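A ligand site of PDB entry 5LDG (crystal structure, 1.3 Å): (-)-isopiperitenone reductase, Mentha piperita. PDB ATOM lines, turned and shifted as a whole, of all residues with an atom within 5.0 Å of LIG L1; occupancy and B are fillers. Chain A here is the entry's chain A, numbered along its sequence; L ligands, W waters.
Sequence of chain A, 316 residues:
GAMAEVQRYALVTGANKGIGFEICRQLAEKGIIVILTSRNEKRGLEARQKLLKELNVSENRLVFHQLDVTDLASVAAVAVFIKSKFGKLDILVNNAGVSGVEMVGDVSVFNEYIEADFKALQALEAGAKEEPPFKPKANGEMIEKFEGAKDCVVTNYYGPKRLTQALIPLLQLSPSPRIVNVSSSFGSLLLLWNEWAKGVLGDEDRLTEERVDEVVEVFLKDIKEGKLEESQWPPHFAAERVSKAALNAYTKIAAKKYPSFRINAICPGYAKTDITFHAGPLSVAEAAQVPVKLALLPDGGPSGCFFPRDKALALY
The backbone NH (N) of Val 69 lies within hydrogen-bond range of a nitrogen (N4) of LIG L1, 3.2 Å away.
N3 of LIG L1 sits at hydrogen-bond distance from OD1 of Asp 68 (2.9 Å).
An oxygen (O12) of LIG L1 lies within hydrogen-bond range of the side-chain amino group (NZ) of Lys 244 (3.0 Å).
O17 of LIG L1 lies within salt-bridge range of NH2 of Arg 43, at 2.9 Å.
The backbone carbonyl oxygen (O) of Gly 14 is in hydrogen-bond range of an oxygen (O5) of LIG L1 (3.2 Å).
O of Asn 95 lies within hydrogen-bond range of O12 of LIG L1, at 2.8 Å.
O14 of LIG L1 sits at hydrogen-bond distance from N of Ala 271 (2.8 Å).
NE of Arg 39 is in salt-bridge range of O17 of LIG L1.
OG1 of Thr 273 lies within hydrogen-bond range of O9 of LIG L1, at 2.8 Å.
OG of Ser 184 lies within hydrogen-bond range of O1 of LG2 L2, at 2.6 Å.
O1 of LG2 L2 lies close to OE2 of Glu 240 (2.5 Å).
An oxygen (O8) of LIG L1 is in hydrogen-bond range of the backbone NH (N) of Ile 19, 2.9 Å away.
O15 of LIG L1 lies within salt-bridge range of NZ of Lys 17, at 3.9 Å.
An oxygen (O5) of LIG L1 lies within hydrogen-bond range of the side-chain amide oxygen (OD1) of Asn 16 (2.8 Å).
O of Ala 271 sits at hydrogen-bond distance from N7 of LIG L1, 3.2 Å away.
O14 of LIG L1 sits close to O of Gly 269, at 3.4 Å.
Ala 15 touches LIG L1.
Gly 18 touches LIG L1.
O of Leu 67 touches C9 of LIG L1, 3.5 Å away.
CG2 of Thr 70 touches N3 of LIG L1 (3.6 Å).
CB of Ala 96 touches N5 of LIG L1 (3.5 Å).
Gly 97 touches LIG L1.
Val 98 touches LIG L1 (CG1 to N2, 3.6 Å).
Thr 155 touches LIG L1.
Val 182 touches LIG L1.
Ser 183 touches LIG L1.
OE2 of Glu 240 touches O13 of LIG L1 (3.99 Å).
CD of Pro 268 touches C20 of LIG L1 (3.6 Å).
Tyr 270 touches LIG L1 (CA to O14, 3.4 Å).
Asp 274 touches LIG L1.
CG2 of Ile 275 touches O9 of LIG L1, 3.4 Å away.
CG2 of Thr 276 touches O14 of LIG L1, 3.6 Å away.
Hydrophobic or aromatic side chains within 4 Å of LIG L1: Ile 19, Val 69, Ala 96, Val 98, Val 182, Pro 268, Tyr 270 and Ile 275.
Of the 33 residues printed, 29 come within 4 Å of LIG L1.
The nearest printed residue that does not touch LIG L1 is Cys 267 (4.4 Å).
N of Arg 43 is in hydrogen-bond range of OD1 of Asn 40, at 2.9 Å.
The backbone carbonyl oxygen of Gly 14 is in hydrogen-bond range of the side-chain amide nitrogen of Asn 95, 3.0 Å away.
ND2 of Asn 95 sits close to N of Gly 20.
O of Leu 67 sits at hydrogen-bond distance from N of Arg 39 (3.2 Å).
The backbone carbonyl oxygen of Ala 271 lies within hydrogen-bond range of the side-chain hydroxyl of Thr 276, at 3.0 Å.
The backbone NH (N) of Gly 269 sits close to the side-chain sulfur (SG) of Cys 267 (3.6 Å).
OG1 of Thr 273 lies close to N of Ile 275.
The side-chain hydroxyl (OG1) of Thr 276 sits at hydrogen-bond distance from the backbone carbonyl oxygen (O) of Thr 273 (3.1 Å).
Water W4 lies within hydrogen-bond range of O13 of LIG L1, OE1 of Glu 240 and O of Val 98.
Water W5 lies within hydrogen-bond range of an oxygen (O2) of LIG L1 (2.7 Å) and the backbone NH (N) of Asp 274 (2.9 Å).
Water W8 bridges an oxygen (O15) of LIG L1 (2.7 Å) and the side-chain amino group of Lys 17 (2.9 Å).
Water W6 lies within hydrogen-bond range of N5 of LIG L1 (2.8 Å), N of Arg 39 (2.9 Å) and OD1 of Asn 16 (3.0 Å).
Water W3 lies within hydrogen-bond range of the backbone carbonyl oxygen (O) of Gly 97 (2.8 Å) and an oxygen (O1) of LIG L1 (2.9 Å).
Water W2 lies within hydrogen-bond range of OG1 of Thr 155, N2 of LIG L1 and NH1 of Arg 39.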
ATOM      1  N   GLY A  14      -4.433 -17.191  30.479  1.00  0.00           N
ATOM      2  CA  GLY A  14      -4.332 -16.820  29.081  1.00  0.00           C
ATOM      3  C   GLY A  14      -3.874 -17.974  28.211  1.00  0.00           C
ATOM      4  O   GLY A  14      -2.902 -17.845  27.445  1.00  0.00           O
ATOM      5  N   ALA A  15      -4.536 -19.128  28.349  1.00  0.00           N
ATOM      6  CA  ALA A  15      -4.040 -20.370  27.800  1.00  0.00           C
ATOM      7  C   ALA A  15      -4.839 -20.861  26.595  1.00  0.00           C
ATOM      8  O   ALA A  15      -4.594 -21.975  26.112  1.00  0.00           O
ATOM      9  CB  ALA A  15      -3.959 -21.423  28.890  1.00  0.00           C
ATOM     10  N   ASN A  16      -5.790 -20.069  26.090  1.00  0.00           N
ATOM     11  CA  ASN A  16      -6.540 -20.487  24.923  1.00  0.00           C
ATOM     12  C   ASN A  16      -5.780 -20.336  23.631  1.00  0.00           C
ATOM     13  O   ASN A  16      -6.223 -20.886  22.638  1.00  0.00           O
ATOM     14  CB  ASN A  16      -7.886 -19.736  24.823  1.00  0.00           C
ATOM     15  CG  ASN A  16      -7.710 -18.235  24.801  1.00  0.00           C
ATOM     16  OD1 ASN A  16      -7.388 -17.631  25.835  1.00  0.00           O
ATOM     17  ND2 ASN A  16      -7.924 -17.610  23.633  1.00  0.00           N
ATOM     18  N   LYS A  17      -4.672 -19.607  23.602  1.00  0.00           N
ATOM     19  CA  LYS A  17      -3.898 -19.428  22.392  1.00  0.00           C
ATOM     20  C   LYS A  17      -2.496 -18.991  22.789  1.00  0.00           C
ATOM     21  O   LYS A  17      -2.193 -18.785  23.975  1.00  0.00           O
ATOM     22  CB  LYS A  17      -4.573 -18.408  21.461  1.00  0.00           C
ATOM     23  CG  LYS A  17      -4.569 -16.989  21.992  1.00  0.00           C
ATOM     24  CD  LYS A  17      -5.304 -16.053  21.040  1.00  0.00           C
ATOM     25  CE  LYS A  17      -5.196 -14.593  21.455  1.00  0.00           C
ATOM     26  NZ  LYS A  17      -5.831 -13.726  20.442  1.00  0.00           N
ATOM     27  N   GLY A  18      -1.645 -18.847  21.795  1.00  0.00           N
ATOM     28  CA  GLY A  18      -0.355 -18.263  21.986  1.00  0.00           C
ATOM     29  C   GLY A  18       0.569 -19.084  22.866  1.00  0.00           C
ATOM     30  O   GLY A  18       0.502 -20.312  22.923  1.00  0.00           O
ATOM     31  N   ILE A  19       1.451 -18.380  23.562  1.00  0.00           N
ATOM     32  CA  ILE A  19       2.434 -19.048  24.397  1.00  0.00           C
ATOM     33  C   ILE A  19       1.748 -19.873  25.478  1.00  0.00           C
ATOM     34  O   ILE A  19       2.173 -20.983  25.795  1.00  0.00           O
ATOM     35  CB  ILE A  19       3.414 -18.032  25.009  1.00  0.00           C
ATOM     36  CG1 ILE A  19       4.141 -17.250  23.904  1.00  0.00           C
ATOM     37  CG2 ILE A  19       4.394 -18.712  25.945  1.00  0.00           C
ATOM     38  CD1 ILE A  19       5.000 -16.113  24.386  1.00  0.00           C
ATOM     39  N   GLY A  20       0.666 -19.359  26.053  1.00  0.00           N
ATOM     40  CA  GLY A  20       0.001 -20.041  27.142  1.00  0.00           C
ATOM     41  C   GLY A  20      -0.491 -21.421  26.755  1.00  0.00           C
ATOM     42  O   GLY A  20      -0.405 -22.379  27.535  1.00  0.00           O
ATOM     43  N   ARG A  39     -10.288 -16.320  29.611  1.00  0.00           N
ATOM     44  CA  ARG A  39     -11.339 -15.396  30.018  1.00  0.00           C
ATOM     45  C   ARG A  39     -12.652 -15.659  29.314  1.00  0.00           C
ATOM     46  O   ARG A  39     -13.721 -15.416  29.909  1.00  0.00           O
ATOM     47  CB  ARG A  39     -10.921 -13.934  29.844  1.00  0.00           C
ATOM     48  CG  ARG A  39     -10.491 -13.525  28.467  1.00  0.00           C
ATOM     49  CD  ARG A  39     -10.300 -12.020  28.396  1.00  0.00           C
ATOM     50  NE  ARG A  39      -9.626 -11.662  27.167  1.00  0.00           N
ATOM     51  CZ  ARG A  39      -9.270 -10.426  26.844  1.00  0.00           C
ATOM     52  NH1 ARG A  39      -9.551  -9.419  27.639  1.00  0.00           N
ATOM     53  NH2 ARG A  39      -8.587 -10.224  25.727  1.00  0.00           N
ATOM     54  N   ASN A  40     -12.610 -16.138  28.066  1.00  0.00           N
ATOM     55  CA  ASN A  40     -13.800 -16.464  27.297  1.00  0.00           C
ATOM     56  C   ASN A  40     -14.010 -17.973  27.394  1.00  0.00           C
ATOM     57  O   ASN A  40     -13.124 -18.765  27.061  1.00  0.00           O
ATOM     58  CB  ASN A  40     -13.653 -15.989  25.849  1.00  0.00           C
ATOM     59  CG  ASN A  40     -14.864 -16.276  25.022  1.00  0.00           C
ATOM     60  OD1 ASN A  40     -14.979 -17.359  24.467  1.00  0.00           O
ATOM     61  ND2 ASN A  40     -15.784 -15.322  24.949  1.00  0.00           N
ATOM     62  N   ARG A  43     -13.883 -19.977  23.911  1.00  0.00           N
ATOM     63  CA  ARG A  43     -12.520 -20.139  23.413  1.00  0.00           C
ATOM     64  C   ARG A  43     -11.739 -21.132  24.255  1.00  0.00           C
ATOM     65  O   ARG A  43     -10.932 -21.890  23.716  1.00  0.00           O
ATOM     66  CB  ARG A  43     -11.773 -18.801  23.377  1.00  0.00           C
ATOM     67  CG  ARG A  43     -12.253 -17.855  22.278  1.00  0.00           C
ATOM     68  CD  ARG A  43     -11.281 -16.725  21.984  1.00  0.00           C
ATOM     69  NE  ARG A  43     -11.208 -15.692  23.001  1.00  0.00           N
ATOM     70  CZ  ARG A  43     -12.010 -14.632  23.060  1.00  0.00           C
ATOM     71  NH1 ARG A  43     -13.040 -14.535  22.236  1.00  0.00           N
ATOM     72  NH2 ARG A  43     -11.794 -13.705  23.975  1.00  0.00           N
ATOM     73  N   LEU A  67     -11.236 -17.980  33.591  1.00  0.00           N
ATOM     74  CA  LEU A  67     -10.490 -17.054  34.450  1.00  0.00           C
ATOM     75  C   LEU A  67     -10.172 -15.792  33.654  1.00  0.00           C
ATOM     76  O   LEU A  67      -9.427 -15.858  32.662  1.00  0.00           O
ATOM     77  CB  LEU A  67      -9.219 -17.685  34.962  1.00  0.00           C
ATOM     78  CG  LEU A  67      -8.320 -16.751  35.780  1.00  0.00           C
ATOM     79  CD1 LEU A  67      -9.018 -16.208  36.979  1.00  0.00           C
ATOM     80  CD2 LEU A  67      -7.070 -17.543  36.217  1.00  0.00           C
ATOM     81  N   ASP A  68     -10.721 -14.671  34.101  1.00  0.00           N
ATOM     82  CA  ASP A  68     -10.342 -13.339  33.627  1.00  0.00           C
ATOM     83  C   ASP A  68      -9.566 -12.723  34.784  1.00  0.00           C
ATOM     84  O   ASP A  68     -10.142 -12.506  35.855  1.00  0.00           O
ATOM     85  CB  ASP A  68     -11.573 -12.515  33.284  1.00  0.00           C
ATOM     86  CG  ASP A  68     -11.248 -11.154  32.723  1.00  0.00           C
ATOM     87  OD1 ASP A  68     -10.201 -10.595  33.060  1.00  0.00           O
ATOM     88  OD2 ASP A  68     -12.084 -10.644  31.952  1.00  0.00           O
ATOM     89  N   VAL A  69      -8.269 -12.465  34.563  1.00  0.00           N
ATOM     90  CA  VAL A  69      -7.397 -11.996  35.650  1.00  0.00           C
ATOM     91  C   VAL A  69      -7.687 -10.581  36.071  1.00  0.00           C
ATOM     92  O   VAL A  69      -7.109 -10.116  37.049  1.00  0.00           O
ATOM     93  CB  VAL A  69      -5.906 -12.185  35.285  1.00  0.00           C
ATOM     94  CG1 VAL A  69      -5.623 -13.624  34.930  1.00  0.00           C
ATOM     95  CG2 VAL A  69      -5.483 -11.257  34.178  1.00  0.00           C
ATOM     96  N   THR A  70      -8.575  -9.875  35.359  1.00  0.00           N
ATOM     97  CA  THR A  70      -8.977  -8.530  35.731  1.00  0.00           C
ATOM     98  C   THR A  70     -10.283  -8.488  36.493  1.00  0.00           C
ATOM     99  O   THR A  70     -10.751  -7.409  36.841  1.00  0.00           O
ATOM    100  CB  THR A  70      -9.093  -7.596  34.521  1.00  0.00           C
ATOM    101  OG1 THR A  70     -10.236  -7.961  33.741  1.00  0.00           O
ATOM    102  CG2 THR A  70      -7.856  -7.609  33.678  1.00  0.00           C
ATOM    103  N   ASN A  95       0.625 -15.951  32.634  1.00  0.00           N
ATOM    104  CA  ASN A  95       0.940 -15.755  31.224  1.00  0.00           C
ATOM    105  C   ASN A  95       0.072 -14.693  30.549  1.00  0.00           C
ATOM    106  O   ASN A  95       0.550 -14.009  29.644  1.00  0.00           O
ATOM    107  CB  ASN A  95       0.872 -17.103  30.478  1.00  0.00           C
ATOM    108  CG  ASN A  95       0.905 -16.931  28.998  1.00  0.00           C
ATOM    109  OD1 ASN A  95       1.977 -16.789  28.391  1.00  0.00           O
ATOM    110  ND2 ASN A  95      -0.251 -16.954  28.403  1.00  0.00           N
ATOM    111  N   ALA A  96      -1.192 -14.559  30.944  1.00  0.00           N
ATOM    112  CA  ALA A  96      -2.072 -13.610  30.281  1.00  0.00           C
ATOM    113  C   ALA A  96      -1.435 -12.227  30.204  1.00  0.00           C
ATOM    114  O   ALA A  96      -0.859 -11.736  31.166  1.00  0.00           O
ATOM    115  CB  ALA A  96      -3.364 -13.494  31.064  1.00  0.00           C
ATOM    116  N   GLY A  97      -1.610 -11.548  29.067  1.00  0.00           N
ATOM    117  CA  GLY A  97      -1.070 -10.220  28.906  1.00  0.00           C
ATOM    118  C   GLY A  97      -1.677  -9.568  27.690  1.00  0.00           C
ATOM    119  O   GLY A  97      -2.126 -10.241  26.750  1.00  0.00           O
ATOM    120  N   VAL A  98      -1.616  -8.233  27.678  1.00  0.00           N
ATOM    121  CA  VAL A  98      -2.022  -7.418  26.541  1.00  0.00           C
ATOM    122  C   VAL A  98      -0.982  -6.308  26.350  1.00  0.00           C
ATOM    123  O   VAL A  98      -0.214  -6.003  27.241  1.00  0.00           O
ATOM    124  CB  VAL A  98      -3.441  -6.812  26.716  1.00  0.00           C
ATOM    125  CG1 VAL A  98      -4.489  -7.920  26.822  1.00  0.00           C
ATOM    126  CG2 VAL A  98      -3.493  -5.903  27.899  1.00  0.00           C
ATOM    127  N   THR A 155      -4.227  -5.934  33.590  1.00  0.00           N
ATOM    128  CA  THR A 155      -4.015  -7.307  33.153  1.00  0.00           C
ATOM    129  C   THR A 155      -2.623  -7.794  33.545  1.00  0.00           C
ATOM    130  O   THR A 155      -2.464  -8.921  34.016  1.00  0.00           O
ATOM    131  CB  THR A 155      -4.183  -7.442  31.644  1.00  0.00           C
ATOM    132  OG1 THR A 155      -5.478  -6.981  31.254  1.00  0.00           O
ATOM    133  CG2 THR A 155      -4.058  -8.869  31.198  1.00  0.00           C
ATOM    134  N   VAL A 182       5.247 -14.396  33.305  1.00  0.00           N
ATOM    135  CA  VAL A 182       5.698 -14.173  31.928  1.00  0.00           C
ATOM    136  C   VAL A 182       5.776 -12.672  31.751  1.00  0.00           C
ATOM    137  O   VAL A 182       4.765 -11.975  31.629  1.00  0.00           O
ATOM    138  CB  VAL A 182       4.776 -14.827  30.891  1.00  0.00           C
ATOM    139  CG1 VAL A 182       5.323 -14.578  29.487  1.00  0.00           C
ATOM    140  CG2 VAL A 182       4.608 -16.317  31.148  1.00  0.00           C
ATOM    141  N   SER A 183       6.989 -12.157  31.764  1.00  0.00           N
ATOM    142  CA  SER A 183       7.286 -10.750  31.710  1.00  0.00           C
ATOM    143  C   SER A 183       7.901 -10.438  30.345  1.00  0.00           C
ATOM    144  O   SER A 183       7.544 -11.086  29.355  1.00  0.00           O
ATOM    145  CB  SER A 183       8.142 -10.367  32.910  1.00  0.00           C
ATOM    146  OG  SER A 183       8.278  -8.977  32.936  1.00  0.00           O
ATOM    147  N   SER A 184       8.763  -9.453  30.288  1.00  0.00           N
ATOM    148  CA  SER A 184       9.374  -9.042  29.051  1.00  0.00           C
ATOM    149  C   SER A 184      10.692  -8.373  29.383  1.00  0.00           C
ATOM    150  O   SER A 184      10.770  -7.636  30.350  1.00  0.00           O
ATOM    151  CB  SER A 184       8.491  -7.999  28.315  1.00  0.00           C
ATOM    152  OG  SER A 184       9.189  -7.482  27.225  1.00  0.00           O
ATOM    153  N   GLU A 240       3.115  -1.054  28.450  1.00  0.00           N
ATOM    154  CA  GLU A 240       3.766  -2.354  28.471  1.00  0.00           C
ATOM    155  C   GLU A 240       5.030  -2.308  29.323  1.00  0.00           C
ATOM    156  O   GLU A 240       5.263  -3.194  30.159  1.00  0.00           O
ATOM    157  CB  GLU A 240       4.075  -2.797  27.032  1.00  0.00           C
ATOM    158  CG  GLU A 240       4.942  -4.056  26.917  1.00  0.00           C
ATOM    159  CD  GLU A 240       4.284  -5.344  27.316  1.00  0.00           C
ATOM    160  OE1 GLU A 240       3.076  -5.323  27.612  1.00  0.00           O
ATOM    161  OE2 GLU A 240       4.976  -6.391  27.281  1.00  0.00           O
ATOM    162  N   LYS A 244       5.308  -4.310  32.903  1.00  0.00           N
ATOM    163  CA  LYS A 244       6.269  -5.404  33.044  1.00  0.00           C
ATOM    164  C   LYS A 244       7.363  -5.073  34.057  1.00  0.00           C
ATOM    165  O   LYS A 244       7.806  -5.953  34.810  1.00  0.00           O
ATOM    166  CB  LYS A 244       6.817  -5.820  31.678  1.00  0.00           C
ATOM    167  CG  LYS A 244       5.779  -6.379  30.726  1.00  0.00           C
ATOM    168  CD  LYS A 244       5.144  -7.662  31.120  1.00  0.00           C
ATOM    169  CE  LYS A 244       4.431  -8.329  29.932  1.00  0.00           C
ATOM    170  NZ  LYS A 244       3.742  -9.637  30.279  1.00  0.00           N
ATOM    171  N   CYS A 267      11.485 -13.717  30.319  1.00  0.00           N
ATOM    172  CA  CYS A 267      11.125 -13.278  28.974  1.00  0.00           C
ATOM    173  C   CYS A 267      11.196 -14.490  28.067  1.00  0.00           C
ATOM    174  O   CYS A 267      12.239 -15.159  28.013  1.00  0.00           O
ATOM    175  CB  CYS A 267      12.075 -12.183  28.459  1.00  0.00           C
ATOM    176  SG  CYS A 267      11.647 -11.544  26.824  1.00  0.00           S
ATOM    177  N   PRO A 268      10.146 -14.758  27.298  1.00  0.00           N
ATOM    178  CA  PRO A 268      10.137 -15.961  26.451  1.00  0.00           C
ATOM    179  C   PRO A 268      10.925 -15.802  25.176  1.00  0.00           C
ATOM    180  O   PRO A 268      11.152 -16.811  24.495  1.00  0.00           O
ATOM    181  CB  PRO A 268       8.644 -16.134  26.152  1.00  0.00           C
ATOM    182  CG  PRO A 268       8.095 -14.757  26.159  1.00  0.00           C
ATOM    183  CD  PRO A 268       8.855 -14.043  27.231  1.00  0.00           C
ATOM    184  N   GLY A 269      11.299 -14.575  24.822  1.00  0.00           N
ATOM    185  CA  GLY A 269      11.820 -14.253  23.514  1.00  0.00           C
ATOM    186  C   GLY A 269      10.725 -13.706  22.629  1.00  0.00           C
ATOM    187  O   GLY A 269       9.550 -13.725  22.952  1.00  0.00           O
ATOM    188  N   TYR A 270      11.127 -13.261  21.464  1.00  0.00           N
ATOM    189  CA  TYR A 270      10.234 -12.600  20.509  1.00  0.00           C
ATOM    190  C   TYR A 270       9.649 -13.717  19.634  1.00  0.00           C
ATOM    191  O   TYR A 270      10.373 -14.365  18.854  1.00  0.00           O
ATOM    192  CB  TYR A 270      11.067 -11.599  19.728  1.00  0.00           C
ATOM    193  CG  TYR A 270      10.360 -10.786  18.699  1.00  0.00           C
ATOM    194  CD1 TYR A 270       8.974 -10.634  18.688  1.00  0.00           C
ATOM    195  CD2 TYR A 270      11.101 -10.118  17.716  1.00  0.00           C
ATOM    196  CE1 TYR A 270       8.342  -9.856  17.707  1.00  0.00           C
ATOM    197  CE2 TYR A 270      10.479  -9.347  16.756  1.00  0.00           C
ATOM    198  CZ  TYR A 270       9.115  -9.206  16.778  1.00  0.00           C
ATOM    199  OH  TYR A 270       8.506  -8.423  15.792  1.00  0.00           O
ATOM    200  N   ALA A 271       8.343 -13.962  19.783  1.00  0.00           N
ATOM    201  CA  ALA A 271       7.725 -15.159  19.229  1.00  0.00           C
ATOM    202  C   ALA A 271       6.464 -14.815  18.461  1.00  0.00           C
ATOM    203  O   ALA A 271       5.768 -13.847  18.770  1.00  0.00           O
ATOM    204  CB  ALA A 271       7.360 -16.094  20.367  1.00  0.00           C
ATOM    205  N   THR A 273       2.969 -14.730  17.702  1.00  0.00           N
ATOM    206  CA  THR A 273       1.663 -14.917  18.326  1.00  0.00           C
ATOM    207  C   THR A 273       0.758 -13.776  17.872  1.00  0.00           C
ATOM    208  O   THR A 273       1.195 -12.839  17.198  1.00  0.00           O
ATOM    209  CB  THR A 273       1.749 -14.874  19.860  1.00  0.00           C
ATOM    210  OG1 THR A 273       2.060 -13.545  20.241  1.00  0.00           O
ATOM    211  CG2 THR A 273       2.762 -15.824  20.413  1.00  0.00           C
ATOM    212  N   ASP A 274      -0.499 -13.793  18.305  1.00  0.00           N
ATOM    213  CA  ASP A 274      -1.392 -12.700  17.915  1.00  0.00           C
ATOM    214  C   ASP A 274      -0.887 -11.357  18.410  1.00  0.00           C
ATOM    215  O   ASP A 274      -1.069 -10.344  17.740  1.00  0.00           O
ATOM    216  CB  ASP A 274      -2.813 -12.929  18.444  1.00  0.00           C
ATOM    217  CG  ASP A 274      -3.607 -13.907  17.605  1.00  0.00           C
ATOM    218  OD1 ASP A 274      -3.254 -14.173  16.426  1.00  0.00           O
ATOM    219  OD2 ASP A 274      -4.647 -14.356  18.080  1.00  0.00           O
ATOM    220  N   ILE A 275      -0.197 -11.315  19.548  1.00  0.00           N
ATOM    221  CA  ILE A 275       0.251 -10.020  20.082  1.00  0.00           C
ATOM    222  C   ILE A 275       1.300  -9.386  19.182  1.00  0.00           C
ATOM    223  O   ILE A 275       1.434  -8.160  19.158  1.00  0.00           O
ATOM    224  CB  ILE A 275       0.725 -10.163  21.542  1.00  0.00           C
ATOM    225  CG1 ILE A 275       0.525  -8.861  22.299  1.00  0.00           C
ATOM    226  CG2 ILE A 275       2.166 -10.636  21.633  1.00  0.00           C
ATOM    227  CD1 ILE A 275       0.760  -9.016  23.793  1.00  0.00           C
ATOM    228  N   THR A 276       2.073 -10.192  18.446  1.00  0.00           N
ATOM    229  CA  THR A 276       3.100  -9.690  17.551  1.00  0.00           C
ATOM    230  C   THR A 276       2.680  -9.770  16.080  1.00  0.00           C
ATOM    231  O   THR A 276       3.537  -9.619  15.193  1.00  0.00           O
ATOM    232  CB  THR A 276       4.396 -10.472  17.707  1.00  0.00           C
ATOM    233  OG1 THR A 276       4.158 -11.803  17.277  1.00  0.00           O
ATOM    234  CG2 THR A 276       4.969 -10.417  19.098  1.00  0.00           C
HETATM  235  P1  LIG L   1      -1.433 -13.758  22.655  1.00  0.00           P
HETATM  236  O1  LIG L   1      -2.106 -12.478  22.384  1.00  0.00           O
HETATM  237  O2  LIG L   1      -1.431 -14.725  21.689  1.00  0.00           O
HETATM  238  O3  LIG L   1      -2.085 -14.450  23.974  1.00  0.00           O
HETATM  239  C1  LIG L   1      -2.456 -13.606  25.090  1.00  0.00           C
HETATM  240  C2  LIG L   1      -3.329 -14.456  25.951  1.00  0.00           C
HETATM  241  O4  LIG L   1      -3.673 -13.672  27.120  1.00  0.00           O
HETATM  242  C3  LIG L   1      -4.642 -14.875  25.283  1.00  0.00           C
HETATM  243  O5  LIG L   1      -4.996 -16.174  25.759  1.00  0.00           O
HETATM  244  C4  LIG L   1      -5.578 -13.810  25.830  1.00  0.00           C
HETATM  245  O6  LIG L   1      -6.950 -14.220  25.822  1.00  0.00           O
HETATM  246  C5  LIG L   1      -5.067 -13.756  27.250  1.00  0.00           C
HETATM  247  N1  LIG L   1      -5.581 -12.637  28.027  1.00  0.00           N
HETATM  248  C6  LIG L   1      -5.551 -11.291  27.761  1.00  0.00           C
HETATM  249  N2  LIG L   1      -6.181 -10.567  28.662  1.00  0.00           N
HETATM  250  C7  LIG L   1      -6.656 -11.516  29.566  1.00  0.00           C
HETATM  251  C8  LIG L   1      -7.431 -11.403  30.752  1.00  0.00           C
HETATM  252  N3  LIG L   1      -7.962 -10.254  31.199  1.00  0.00           N
HETATM  253  N4  LIG L   1      -7.676 -12.533  31.437  1.00  0.00           N
HETATM  254  C9  LIG L   1      -7.251 -13.698  30.955  1.00  0.00           C
HETATM  255  N5  LIG L   1      -6.567 -13.927  29.829  1.00  0.00           N
HETATM  256  C10 LIG L   1      -6.290 -12.774  29.187  1.00  0.00           C
HETATM  257  O7  LIG L   1       0.051 -13.381  23.022  1.00  0.00           O
HETATM  258  P2  LIG L   1       1.278 -14.137  23.694  1.00  0.00           P
HETATM  259  O8  LIG L   1       0.988 -15.567  23.775  1.00  0.00           O
HETATM  260  O9  LIG L   1       2.487 -13.699  22.966  1.00  0.00           O
HETATM  261  O10 LIG L   1       1.222 -13.498  25.146  1.00  0.00           O
HETATM  262  C11 LIG L   1       1.505 -14.312  26.333  1.00  0.00           C
HETATM  263  C12 LIG L   1       2.428 -13.558  27.238  1.00  0.00           C
HETATM  264  O11 LIG L   1       3.751 -13.475  26.634  1.00  0.00           O
HETATM  265  C13 LIG L   1       2.000 -12.098  27.518  1.00  0.00           C
HETATM  266  O12 LIG L   1       2.138 -11.799  28.924  1.00  0.00           O
HETATM  267  C14 LIG L   1       3.029 -11.274  26.743  1.00  0.00           C
HETATM  268  O13 LIG L   1       3.300 -10.008  27.320  1.00  0.00           O
HETATM  269  C15 LIG L   1       4.243 -12.180  26.842  1.00  0.00           C
HETATM  270  N6  LIG L   1       5.333 -11.926  25.858  1.00  0.00           N
HETATM  271  C16 LIG L   1       5.152 -12.256  24.561  1.00  0.00           C
HETATM  272  C17 LIG L   1       6.165 -12.044  23.656  1.00  0.00           C
HETATM  273  C18 LIG L   1       6.084 -12.436  22.217  1.00  0.00           C
HETATM  274  O14 LIG L   1       7.019 -12.107  21.462  1.00  0.00           O
HETATM  275  N7  LIG L   1       5.044 -13.095  21.784  1.00  0.00           N
HETATM  276  C19 LIG L   1       7.375 -11.482  24.109  1.00  0.00           C
HETATM  277  C20 LIG L   1       7.527 -11.154  25.453  1.00  0.00           C
HETATM  278  C21 LIG L   1       6.481 -11.388  26.314  1.00  0.00           C
HETATM  279  P3  LIG L   1      -7.979 -13.798  24.626  1.00  0.00           P
HETATM  280  O15 LIG L   1      -7.867 -14.775  23.596  1.00  0.00           O
HETATM  281  O16 LIG L   1      -7.600 -12.432  24.191  1.00  0.00           O
HETATM  282  O17 LIG L   1      -9.281 -13.811  25.345  1.00  0.00           O
HETATM  283  C1  LG2 L   2       5.233  -7.476  24.473  1.00  0.00           C
HETATM  284  C2  LG2 L   2       4.969  -8.681  23.546  1.00  0.00           C
HETATM  285  C3  LG2 L   2       6.002  -8.700  22.422  1.00  0.00           C
HETATM  286  C4  LG2 L   2       4.831  -6.200  23.762  1.00  0.00           C
HETATM  287  C5  LG2 L   2       3.535  -5.833  23.705  1.00  0.00           C
HETATM  288  C6  LG2 L   2       5.899  -5.339  23.192  1.00  0.00           C
HETATM  289  C7  LG2 L   2       8.499  -9.023  21.968  1.00  0.00           C
HETATM  290  O1  LG2 L   2       7.032  -6.758  25.894  1.00  0.00           O
HETATM  291  C8  LG2 L   2       7.412  -8.597  22.907  1.00  0.00           C
HETATM  292  C9  LG2 L   2       7.686  -8.057  24.095  1.00  0.00           C
HETATM  293  C10 LG2 L   2       6.692  -7.447  24.940  1.00  0.00           C
HETATM  294  O   HOH W   1     -10.342 -16.212  26.120  1.00  0.00           O
HETATM  295  O   HOH W   2      -7.174  -7.975  29.410  1.00  0.00           O
HETATM  296  O   HOH W   3      -2.701 -10.202  24.022  1.00  0.00           O
HETATM  297  O   HOH W   4       2.021  -7.757  26.831  1.00  0.00           O
HETATM  298  O   HOH W   5      -1.740 -16.135  19.406  1.00  0.00           O
HETATM  299  O   HOH W   6      -7.782 -15.959  28.287  1.00  0.00           O
HETATM  300  O   HOH W   7      -8.919 -11.135  22.229  1.00  0.00           O
HETATM  301  O   HOH W   8      -8.530 -14.598  20.967  1.00  0.00           O
HETATM  302  O   HOH W   9      -0.660 -16.875  25.538  1.00  0.00           O
